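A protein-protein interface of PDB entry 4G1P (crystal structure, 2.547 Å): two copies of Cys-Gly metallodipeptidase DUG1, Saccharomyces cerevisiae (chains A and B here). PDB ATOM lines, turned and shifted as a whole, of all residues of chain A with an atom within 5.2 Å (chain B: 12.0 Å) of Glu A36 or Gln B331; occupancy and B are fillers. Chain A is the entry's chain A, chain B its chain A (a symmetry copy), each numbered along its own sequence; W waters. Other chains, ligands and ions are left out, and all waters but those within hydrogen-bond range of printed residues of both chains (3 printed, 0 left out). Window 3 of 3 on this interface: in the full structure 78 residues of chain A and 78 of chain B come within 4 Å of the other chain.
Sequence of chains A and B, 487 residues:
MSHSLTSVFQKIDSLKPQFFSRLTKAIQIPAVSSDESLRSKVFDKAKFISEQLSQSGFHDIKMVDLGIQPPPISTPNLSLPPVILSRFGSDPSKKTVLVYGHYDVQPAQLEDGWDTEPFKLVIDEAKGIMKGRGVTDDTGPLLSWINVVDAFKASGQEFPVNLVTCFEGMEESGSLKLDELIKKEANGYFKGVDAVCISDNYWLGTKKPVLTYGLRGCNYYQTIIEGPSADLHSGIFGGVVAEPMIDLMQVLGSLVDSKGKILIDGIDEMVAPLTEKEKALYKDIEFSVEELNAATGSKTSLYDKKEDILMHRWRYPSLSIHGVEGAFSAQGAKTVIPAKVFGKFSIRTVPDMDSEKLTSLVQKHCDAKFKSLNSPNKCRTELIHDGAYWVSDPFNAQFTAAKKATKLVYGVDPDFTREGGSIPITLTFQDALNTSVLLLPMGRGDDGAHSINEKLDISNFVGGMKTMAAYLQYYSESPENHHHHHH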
ATOM      1  N   SER A  34      21.677  -4.942  28.252  1.00  0.00           N
ATOM      2  CA  SER A  34      21.072  -6.137  27.704  1.00  0.00           C
ATOM      3  C   SER A  34      20.760  -5.935  26.235  1.00  0.00           C
ATOM      4  O   SER A  34      20.370  -6.873  25.559  1.00  0.00           O
ATOM      5  CB  SER A  34      19.775  -6.452  28.436  1.00  0.00           C
ATOM      6  OG  SER A  34      18.821  -5.415  28.226  1.00  0.00           O
ATOM      7  N   ASP A  35      20.924  -4.704  25.756  1.00  0.00           N
ATOM      8  CA  ASP A  35      20.560  -4.335  24.393  1.00  0.00           C
ATOM      9  C   ASP A  35      21.794  -4.072  23.534  1.00  0.00           C
ATOM     10  O   ASP A  35      22.460  -3.047  23.687  1.00  0.00           O
ATOM     11  CB  ASP A  35      19.668  -3.087  24.410  1.00  0.00           C
ATOM     12  CG  ASP A  35      19.051  -2.777  23.046  1.00  0.00           C
ATOM     13  OD1 ASP A  35      19.722  -2.955  22.009  1.00  0.00           O
ATOM     14  OD2 ASP A  35      17.882  -2.350  23.008  1.00  0.00           O
ATOM     15  N   GLU A  36      22.071  -4.976  22.602  1.00  0.00           N
ATOM     16  CA  GLU A  36      23.288  -4.882  21.796  1.00  0.00           C
ATOM     17  C   GLU A  36      23.378  -3.582  21.006  1.00  0.00           C
ATOM     18  O   GLU A  36      24.455  -2.993  20.892  1.00  0.00           O
ATOM     19  CB  GLU A  36      23.401  -6.070  20.848  1.00  0.00           C
ATOM     20  CG  GLU A  36      23.723  -7.377  21.528  1.00  0.00           C
ATOM     21  CD  GLU A  36      23.772  -8.521  20.540  1.00  0.00           C
ATOM     22  OE1 GLU A  36      23.746  -8.242  19.312  1.00  0.00           O
ATOM     23  OE2 GLU A  36      23.828  -9.691  20.991  1.00  0.00           O
ATOM     24  N   SER A  37      22.239  -3.136  20.479  1.00  0.00           N
ATOM     25  CA  SER A  37      22.172  -1.903  19.704  1.00  0.00           C
ATOM     26  C   SER A  37      22.511  -0.667  20.537  1.00  0.00           C
ATOM     27  O   SER A  37      22.788   0.395  19.988  1.00  0.00           O
ATOM     28  CB  SER A  37      20.782  -1.734  19.100  1.00  0.00           C
ATOM     29  OG  SER A  37      19.894  -1.147  20.043  1.00  0.00           O
ATOM     30  N   LEU A  38      22.495  -0.802  21.861  1.00  0.00           N
ATOM     31  CA  LEU A  38      22.776   0.329  22.737  1.00  0.00           C
ATOM     32  C   LEU A  38      24.110   0.182  23.446  1.00  0.00           C
ATOM     33  O   LEU A  38      24.435   0.981  24.329  1.00  0.00           O
ATOM     34  CB  LEU A  38      21.669   0.478  23.779  1.00  0.00           C
ATOM     35  CG  LEU A  38      20.263   0.785  23.268  1.00  0.00           C
ATOM     36  CD1 LEU A  38      19.291   0.839  24.423  1.00  0.00           C
ATOM     37  CD2 LEU A  38      20.245   2.085  22.487  1.00  0.00           C
ATOM     38  N   ARG A  39      24.874  -0.846  23.080  1.00  0.00           N
ATOM     39  CA  ARG A  39      26.156  -1.085  23.731  1.00  0.00           C
ATOM     40  C   ARG A  39      27.014   0.179  23.698  1.00  0.00           C
ATOM     41  O   ARG A  39      27.655   0.529  24.688  1.00  0.00           O
ATOM     42  CB  ARG A  39      26.888  -2.273  23.092  1.00  0.00           C
ATOM     43  CG  ARG A  39      28.271  -2.591  23.675  1.00  0.00           C
ATOM     44  CD  ARG A  39      28.241  -2.884  25.176  1.00  0.00           C
ATOM     45  NE  ARG A  39      27.165  -3.804  25.528  1.00  0.00           N
ATOM     46  CZ  ARG A  39      27.328  -5.096  25.799  1.00  0.00           C
ATOM     47  NH1 ARG A  39      28.531  -5.635  25.781  1.00  0.00           N
ATOM     48  NH2 ARG A  39      26.283  -5.853  26.095  1.00  0.00           N
ATOM     49  N   SER A  40      26.984   0.887  22.573  1.00  0.00           N
ATOM     50  CA  SER A  40      27.766   2.111  22.422  1.00  0.00           C
ATOM     51  C   SER A  40      27.355   3.162  23.448  1.00  0.00           C
ATOM     52  O   SER A  40      28.189   3.900  23.960  1.00  0.00           O
ATOM     53  CB  SER A  40      27.646   2.672  21.005  1.00  0.00           C
ATOM     54  OG  SER A  40      26.420   3.336  20.832  1.00  0.00           O
ATOM     55  N   SER A  74      24.990 -15.441  22.613  1.00  0.00           N
ATOM     56  CA  SER A  74      24.901 -14.680  21.373  1.00  0.00           C
ATOM     57  C   SER A  74      25.669 -13.369  21.474  1.00  0.00           C
ATOM     58  O   SER A  74      25.254 -12.450  22.177  1.00  0.00           O
ATOM     59  CB  SER A  74      23.440 -14.404  21.017  1.00  0.00           C
ATOM     60  OG  SER A  74      23.333 -13.329  20.100  1.00  0.00           O
ATOM     61  N   THR A  75      26.789 -13.288  20.767  1.00  0.00           N
ATOM     62  CA  THR A  75      27.599 -12.077  20.758  1.00  0.00           C
ATOM     63  C   THR A  75      28.451 -11.994  19.499  1.00  0.00           C
ATOM     64  O   THR A  75      29.195 -12.919  19.178  1.00  0.00           O
ATOM     65  CB  THR A  75      28.519 -11.999  21.990  1.00  0.00           C
ATOM     66  OG1 THR A  75      29.309 -10.807  21.923  1.00  0.00           O
ATOM     67  CG2 THR A  75      29.438 -13.208  22.043  1.00  0.00           C
ATOM     68  N   PRO A  76      28.331 -10.878  18.789  1.00  0.00           N
ATOM     69  CA  PRO A  76      29.124 -10.639  17.581  1.00  0.00           C
ATOM     70  C   PRO A  76      30.477 -10.056  17.947  1.00  0.00           C
ATOM     71  O   PRO A  76      30.882  -9.043  17.386  1.00  0.00           O
ATOM     72  CB  PRO A  76      28.301  -9.593  16.835  1.00  0.00           C
ATOM     73  CG  PRO A  76      27.588  -8.852  17.911  1.00  0.00           C
ATOM     74  CD  PRO A  76      27.267  -9.875  18.960  1.00  0.00           C
ATOM     75  N   LEU A  78      31.142  -8.448  20.565  1.00  0.00           N
ATOM     76  CA  LEU A  78      30.895  -7.197  21.247  1.00  0.00           C
ATOM     77  C   LEU A  78      31.793  -7.127  22.489  1.00  0.00           C
ATOM     78  O   LEU A  78      31.832  -8.076  23.274  1.00  0.00           O
ATOM     79  CB  LEU A  78      29.429  -7.188  21.665  1.00  0.00           C
ATOM     80  CG  LEU A  78      28.681  -5.877  21.846  1.00  0.00           C
ATOM     81  CD1 LEU A  78      28.625  -5.106  20.540  1.00  0.00           C
ATOM     82  CD2 LEU A  78      27.288  -6.225  22.304  1.00  0.00           C
ATOM     83  N   GLU A 325      10.126 -16.584  25.313  1.00  0.00           N
ATOM     84  CA  GLU A 325      10.800 -16.093  24.121  1.00  0.00           C
ATOM     85  C   GLU A 325      10.562 -17.030  22.922  1.00  0.00           C
ATOM     86  O   GLU A 325      10.668 -18.252  23.049  1.00  0.00           O
ATOM     87  CB  GLU A 325      12.300 -15.968  24.403  1.00  0.00           C
ATOM     88  CG  GLU A 325      13.162 -15.611  23.199  1.00  0.00           C
ATOM     89  CD  GLU A 325      14.647 -15.810  23.479  1.00  0.00           C
ATOM     90  OE1 GLU A 325      15.025 -15.821  24.670  1.00  0.00           O
ATOM     91  OE2 GLU A 325      15.437 -15.964  22.518  1.00  0.00           O
ATOM     92  N   LYS A 344      11.230 -18.568  30.487  1.00  0.00           N
ATOM     93  CA  LYS A 344      12.122 -17.861  31.403  1.00  0.00           C
ATOM     94  C   LYS A 344      11.635 -17.942  32.854  1.00  0.00           C
ATOM     95  O   LYS A 344      10.488 -17.612  33.162  1.00  0.00           O
ATOM     96  CB  LYS A 344      12.268 -16.399  30.969  1.00  0.00           C
ATOM     97  CG  LYS A 344      12.684 -16.219  29.504  1.00  0.00           C
ATOM     98  CD  LYS A 344      14.077 -16.766  29.263  1.00  0.00           C
ATOM     99  CE  LYS A 344      14.495 -16.655  27.815  1.00  0.00           C
ATOM    100  NZ  LYS A 344      14.474 -15.267  27.340  1.00  0.00           N
ATOM    101  N   GLN B 109       9.831 -10.207   9.421  1.00  0.00           N
ATOM    102  CA  GLN B 109      11.119  -9.549   9.586  1.00  0.00           C
ATOM    103  C   GLN B 109      12.205 -10.534   9.247  1.00  0.00           C
ATOM    104  O   GLN B 109      12.077 -11.729   9.528  1.00  0.00           O
ATOM    105  CB  GLN B 109      11.327  -9.122  11.028  1.00  0.00           C
ATOM    106  CG  GLN B 109      10.643  -7.846  11.422  1.00  0.00           C
ATOM    107  CD  GLN B 109      11.007  -7.479  12.840  1.00  0.00           C
ATOM    108  OE1 GLN B 109      11.472  -8.330  13.603  1.00  0.00           O
ATOM    109  NE2 GLN B 109      10.827  -6.211  13.197  1.00  0.00           N
ATOM    110  N   GLU B 111      15.050 -10.909  10.654  1.00  0.00           N
ATOM    111  CA  GLU B 111      15.629 -11.505  11.842  1.00  0.00           C
ATOM    112  C   GLU B 111      14.821 -12.676  12.381  1.00  0.00           C
ATOM    113  O   GLU B 111      15.311 -13.419  13.239  1.00  0.00           O
ATOM    114  CB  GLU B 111      15.830 -10.448  12.927  1.00  0.00           C
ATOM    115  CG  GLU B 111      16.824  -9.338  12.556  1.00  0.00           C
ATOM    116  CD  GLU B 111      16.302  -8.401  11.452  1.00  0.00           C
ATOM    117  OE1 GLU B 111      15.057  -8.359  11.240  1.00  0.00           O
ATOM    118  OE2 GLU B 111      17.142  -7.722  10.797  1.00  0.00           O
ATOM    119  N   ASP B 112      13.598 -12.857  11.887  1.00  0.00           N
ATOM    120  CA  ASP B 112      12.803 -14.006  12.310  1.00  0.00           C
ATOM    121  C   ASP B 112      13.433 -15.297  11.804  1.00  0.00           C
ATOM    122  O   ASP B 112      13.065 -16.373  12.258  1.00  0.00           O
ATOM    123  CB  ASP B 112      11.360 -13.945  11.797  1.00  0.00           C
ATOM    124  CG  ASP B 112      10.596 -12.734  12.294  1.00  0.00           C
ATOM    125  OD1 ASP B 112      10.996 -12.151  13.325  1.00  0.00           O
ATOM    126  OD2 ASP B 112       9.581 -12.375  11.646  1.00  0.00           O
ATOM    127  N   ALA B 327       4.557  -9.975  29.019  1.00  0.00           N
ATOM    128  CA  ALA B 327       5.635 -10.480  29.854  1.00  0.00           C
ATOM    129  C   ALA B 327       6.982 -10.228  29.200  1.00  0.00           C
ATOM    130  O   ALA B 327       7.125  -9.328  28.362  1.00  0.00           O
ATOM    131  CB  ALA B 327       5.448 -11.957  30.141  1.00  0.00           C
ATOM    132  N   PHE B 328       7.972 -11.016  29.576  1.00  0.00           N
ATOM    133  CA  PHE B 328       9.312 -10.802  29.058  1.00  0.00           C
ATOM    134  C   PHE B 328       9.627 -11.794  27.938  1.00  0.00           C
ATOM    135  O   PHE B 328       9.654 -13.005  28.164  1.00  0.00           O
ATOM    136  CB  PHE B 328      10.348 -10.882  30.182  1.00  0.00           C
ATOM    137  CG  PHE B 328      11.744 -11.000  29.695  1.00  0.00           C
ATOM    138  CD1 PHE B 328      12.353  -9.943  29.034  1.00  0.00           C
ATOM    139  CD2 PHE B 328      12.463 -12.175  29.886  1.00  0.00           C
ATOM    140  CE1 PHE B 328      13.677 -10.057  28.578  1.00  0.00           C
ATOM    141  CE2 PHE B 328      13.782 -12.298  29.428  1.00  0.00           C
ATOM    142  CZ  PHE B 328      14.386 -11.236  28.776  1.00  0.00           C
ATOM    143  N   SER B 329       9.876 -11.280  26.737  1.00  0.00           N
ATOM    144  CA  SER B 329       9.950 -12.148  25.565  1.00  0.00           C
ATOM    145  C   SER B 329      11.198 -11.939  24.707  1.00  0.00           C
ATOM    146  O   SER B 329      11.348 -12.586  23.670  1.00  0.00           O
ATOM    147  CB  SER B 329       8.699 -11.982  24.706  1.00  0.00           C
ATOM    148  OG  SER B 329       8.563 -10.635  24.298  1.00  0.00           O
ATOM    149  N   ALA B 330      12.083 -11.043  25.139  1.00  0.00           N
ATOM    150  CA  ALA B 330      13.332 -10.803  24.415  1.00  0.00           C
ATOM    151  C   ALA B 330      14.342 -11.837  24.841  1.00  0.00           C
ATOM    152  O   ALA B 330      14.066 -12.655  25.720  1.00  0.00           O
ATOM    153  CB  ALA B 330      13.855  -9.427  24.692  1.00  0.00           C
ATOM    154  N   GLN B 331      15.522 -11.812  24.240  1.00  0.00           N
ATOM    155  CA  GLN B 331      16.494 -12.836  24.600  1.00  0.00           C
ATOM    156  C   GLN B 331      17.155 -12.524  25.933  1.00  0.00           C
ATOM    157  O   GLN B 331      17.116 -11.385  26.406  1.00  0.00           O
ATOM    158  CB  GLN B 331      17.522 -13.076  23.495  1.00  0.00           C
ATOM    159  CG  GLN B 331      18.705 -12.146  23.507  1.00  0.00           C
ATOM    160  CD  GLN B 331      19.732 -12.539  22.462  1.00  0.00           C
ATOM    161  OE1 GLN B 331      19.477 -13.408  21.621  1.00  0.00           O
ATOM    162  NE2 GLN B 331      20.897 -11.907  22.510  1.00  0.00           N
ATOM    163  N   GLY B 332      17.728 -13.561  26.540  1.00  0.00           N
ATOM    164  CA  GLY B 332      18.413 -13.433  27.805  1.00  0.00           C
ATOM    165  C   GLY B 332      17.492 -13.418  29.010  1.00  0.00           C
ATOM    166  O   GLY B 332      16.439 -14.070  29.034  1.00  0.00           O
ATOM    167  N   ALA B 333      17.889 -12.650  30.017  1.00  0.00           N
ATOM    168  CA  ALA B 333      17.238 -12.699  31.309  1.00  0.00           C
ATOM    169  C   ALA B 333      16.623 -11.358  31.729  1.00  0.00           C
ATOM    170  O   ALA B 333      17.220 -10.313  31.556  1.00  0.00           O
ATOM    171  CB  ALA B 333      18.237 -13.178  32.339  1.00  0.00           C
ATOM    172  N   LYS B 334      15.415 -11.396  32.275  1.00  0.00           N
ATOM    173  CA  LYS B 334      14.844 -10.230  32.925  1.00  0.00           C
ATOM    174  C   LYS B 334      14.123 -10.662  34.213  1.00  0.00           C
ATOM    175  O   LYS B 334      13.225 -11.512  34.201  1.00  0.00           O
ATOM    176  CB  LYS B 334      13.898  -9.486  31.981  1.00  0.00           C
ATOM    177  CG  LYS B 334      13.503  -8.065  32.425  1.00  0.00           C
ATOM    178  CD  LYS B 334      12.455  -7.494  31.485  1.00  0.00           C
ATOM    179  CE  LYS B 334      12.295  -5.969  31.563  1.00  0.00           C
ATOM    180  NZ  LYS B 334      11.863  -5.378  30.228  1.00  0.00           N
ATOM    181  N   THR B 335      14.540 -10.079  35.329  1.00  0.00           N
ATOM    182  CA  THR B 335      14.019 -10.461  36.629  1.00  0.00           C
ATOM    183  C   THR B 335      12.844  -9.582  36.951  1.00  0.00           C
ATOM    184  O   THR B 335      12.970  -8.596  37.690  1.00  0.00           O
ATOM    185  CB  THR B 335      15.058 -10.290  37.724  1.00  0.00           C
ATOM    186  OG1 THR B 335      15.791  -9.087  37.490  1.00  0.00           O
ATOM    187  CG2 THR B 335      16.019 -11.450  37.740  1.00  0.00           C
ATOM    188  N   VAL B 336      11.695  -9.960  36.409  1.00  0.00           N
ATOM    189  CA  VAL B 336      10.491  -9.163  36.558  1.00  0.00           C
ATOM    190  C   VAL B 336       9.260 -10.040  36.783  1.00  0.00           C
ATOM    191  O   VAL B 336       9.164 -11.148  36.266  1.00  0.00           O
ATOM    192  CB  VAL B 336      10.276  -8.256  35.312  1.00  0.00           C
ATOM    193  CG1 VAL B 336      10.156  -9.100  34.050  1.00  0.00           C
ATOM    194  CG2 VAL B 336       9.061  -7.392  35.493  1.00  0.00           C
HETATM  195  O   HOH W   1      12.135 -14.110  27.079  1.00  0.00           O
HETATM  196  O   HOH W   2      17.952 -16.199  22.100  1.00  0.00           O
HETATM  197  O   HOH W   3      17.677 -16.654  25.503  1.00  0.00           O
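Gln B331 touches Glu A36. Ser A74 touches Gln B331 (OG to NE2, 3.7 Å). Glu A325 touches Ser B329. Gln B331 touches Glu A325 (CA to OE1, 3.3 Å). Glu A325 touches Gly B332 (OE1 to N, 3.99 Å). NZ of Lys A344 touches CE2 of Phe B328, at 3.7 Å.
NZ of Lys A344 is in hydrogen-bond range of O of Ala B330, at 3.1 Å. The side-chain amino group (NZ) of Lys A344 lies within hydrogen-bond range of the backbone carbonyl oxygen (O) of Gly B332 (2.9 Å). The side-chain carboxylate (OE1) of Glu A325 lies close to the backbone carbonyl oxygen (O) of Ala B330 (3.5 Å).
Glu A36 touches just one residue of chain B: Gln B331 (3.98 Å). Gln B331 touches three residues of chain A. No residue of chain B comes within 4 Å of Asp A35. No residue of chain B comes within 4 Å of Ser A37. No residue of chain B comes within 4 Å of Arg A39. Ser A74 touches one residue of chain B. No residue of chain B comes within 4 Å of Thr A75. Of the printed residues of chain A, Ala B330 touches Glu A325 and Lys A344. Of the printed residues of chain B, Glu A325 touches Ser B329, Ala B330, Gln B331 and Gly B332. Of the printed residues of chain A, Ser B329 touches Glu A325. The nearest residue of chain B that does not touch Glu A36 is Gly B332 (9.1 Å). The nearest printed residue of chain B that does not touch Glu A325 is Phe B328 (4.6 Å).
Water W2 bridges OE2 of Glu A325 (2.6 Å) and OE1 of Gln B331 (3.2 Å). Water W1 lies within hydrogen-bond range of the side-chain amino group (NZ) of Lys A344, the backbone carbonyl oxygen (O) of Ala B330 and the backbone carbonyl oxygen (O) of Phe B328. Water W3 lies within hydrogen-bond range of OE1 of Glu A325 and N of Gly B332.
The side-chain amino group (NZ) of Lys A344 lies within salt-bridge range of the side-chain carboxylate (OE1) of Glu A325 (2.8 Å).
No position is printed for both chains. Of the 9 pairs that touch across the chains among the printed residues, none has its exchanged pair printed and touching as well.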
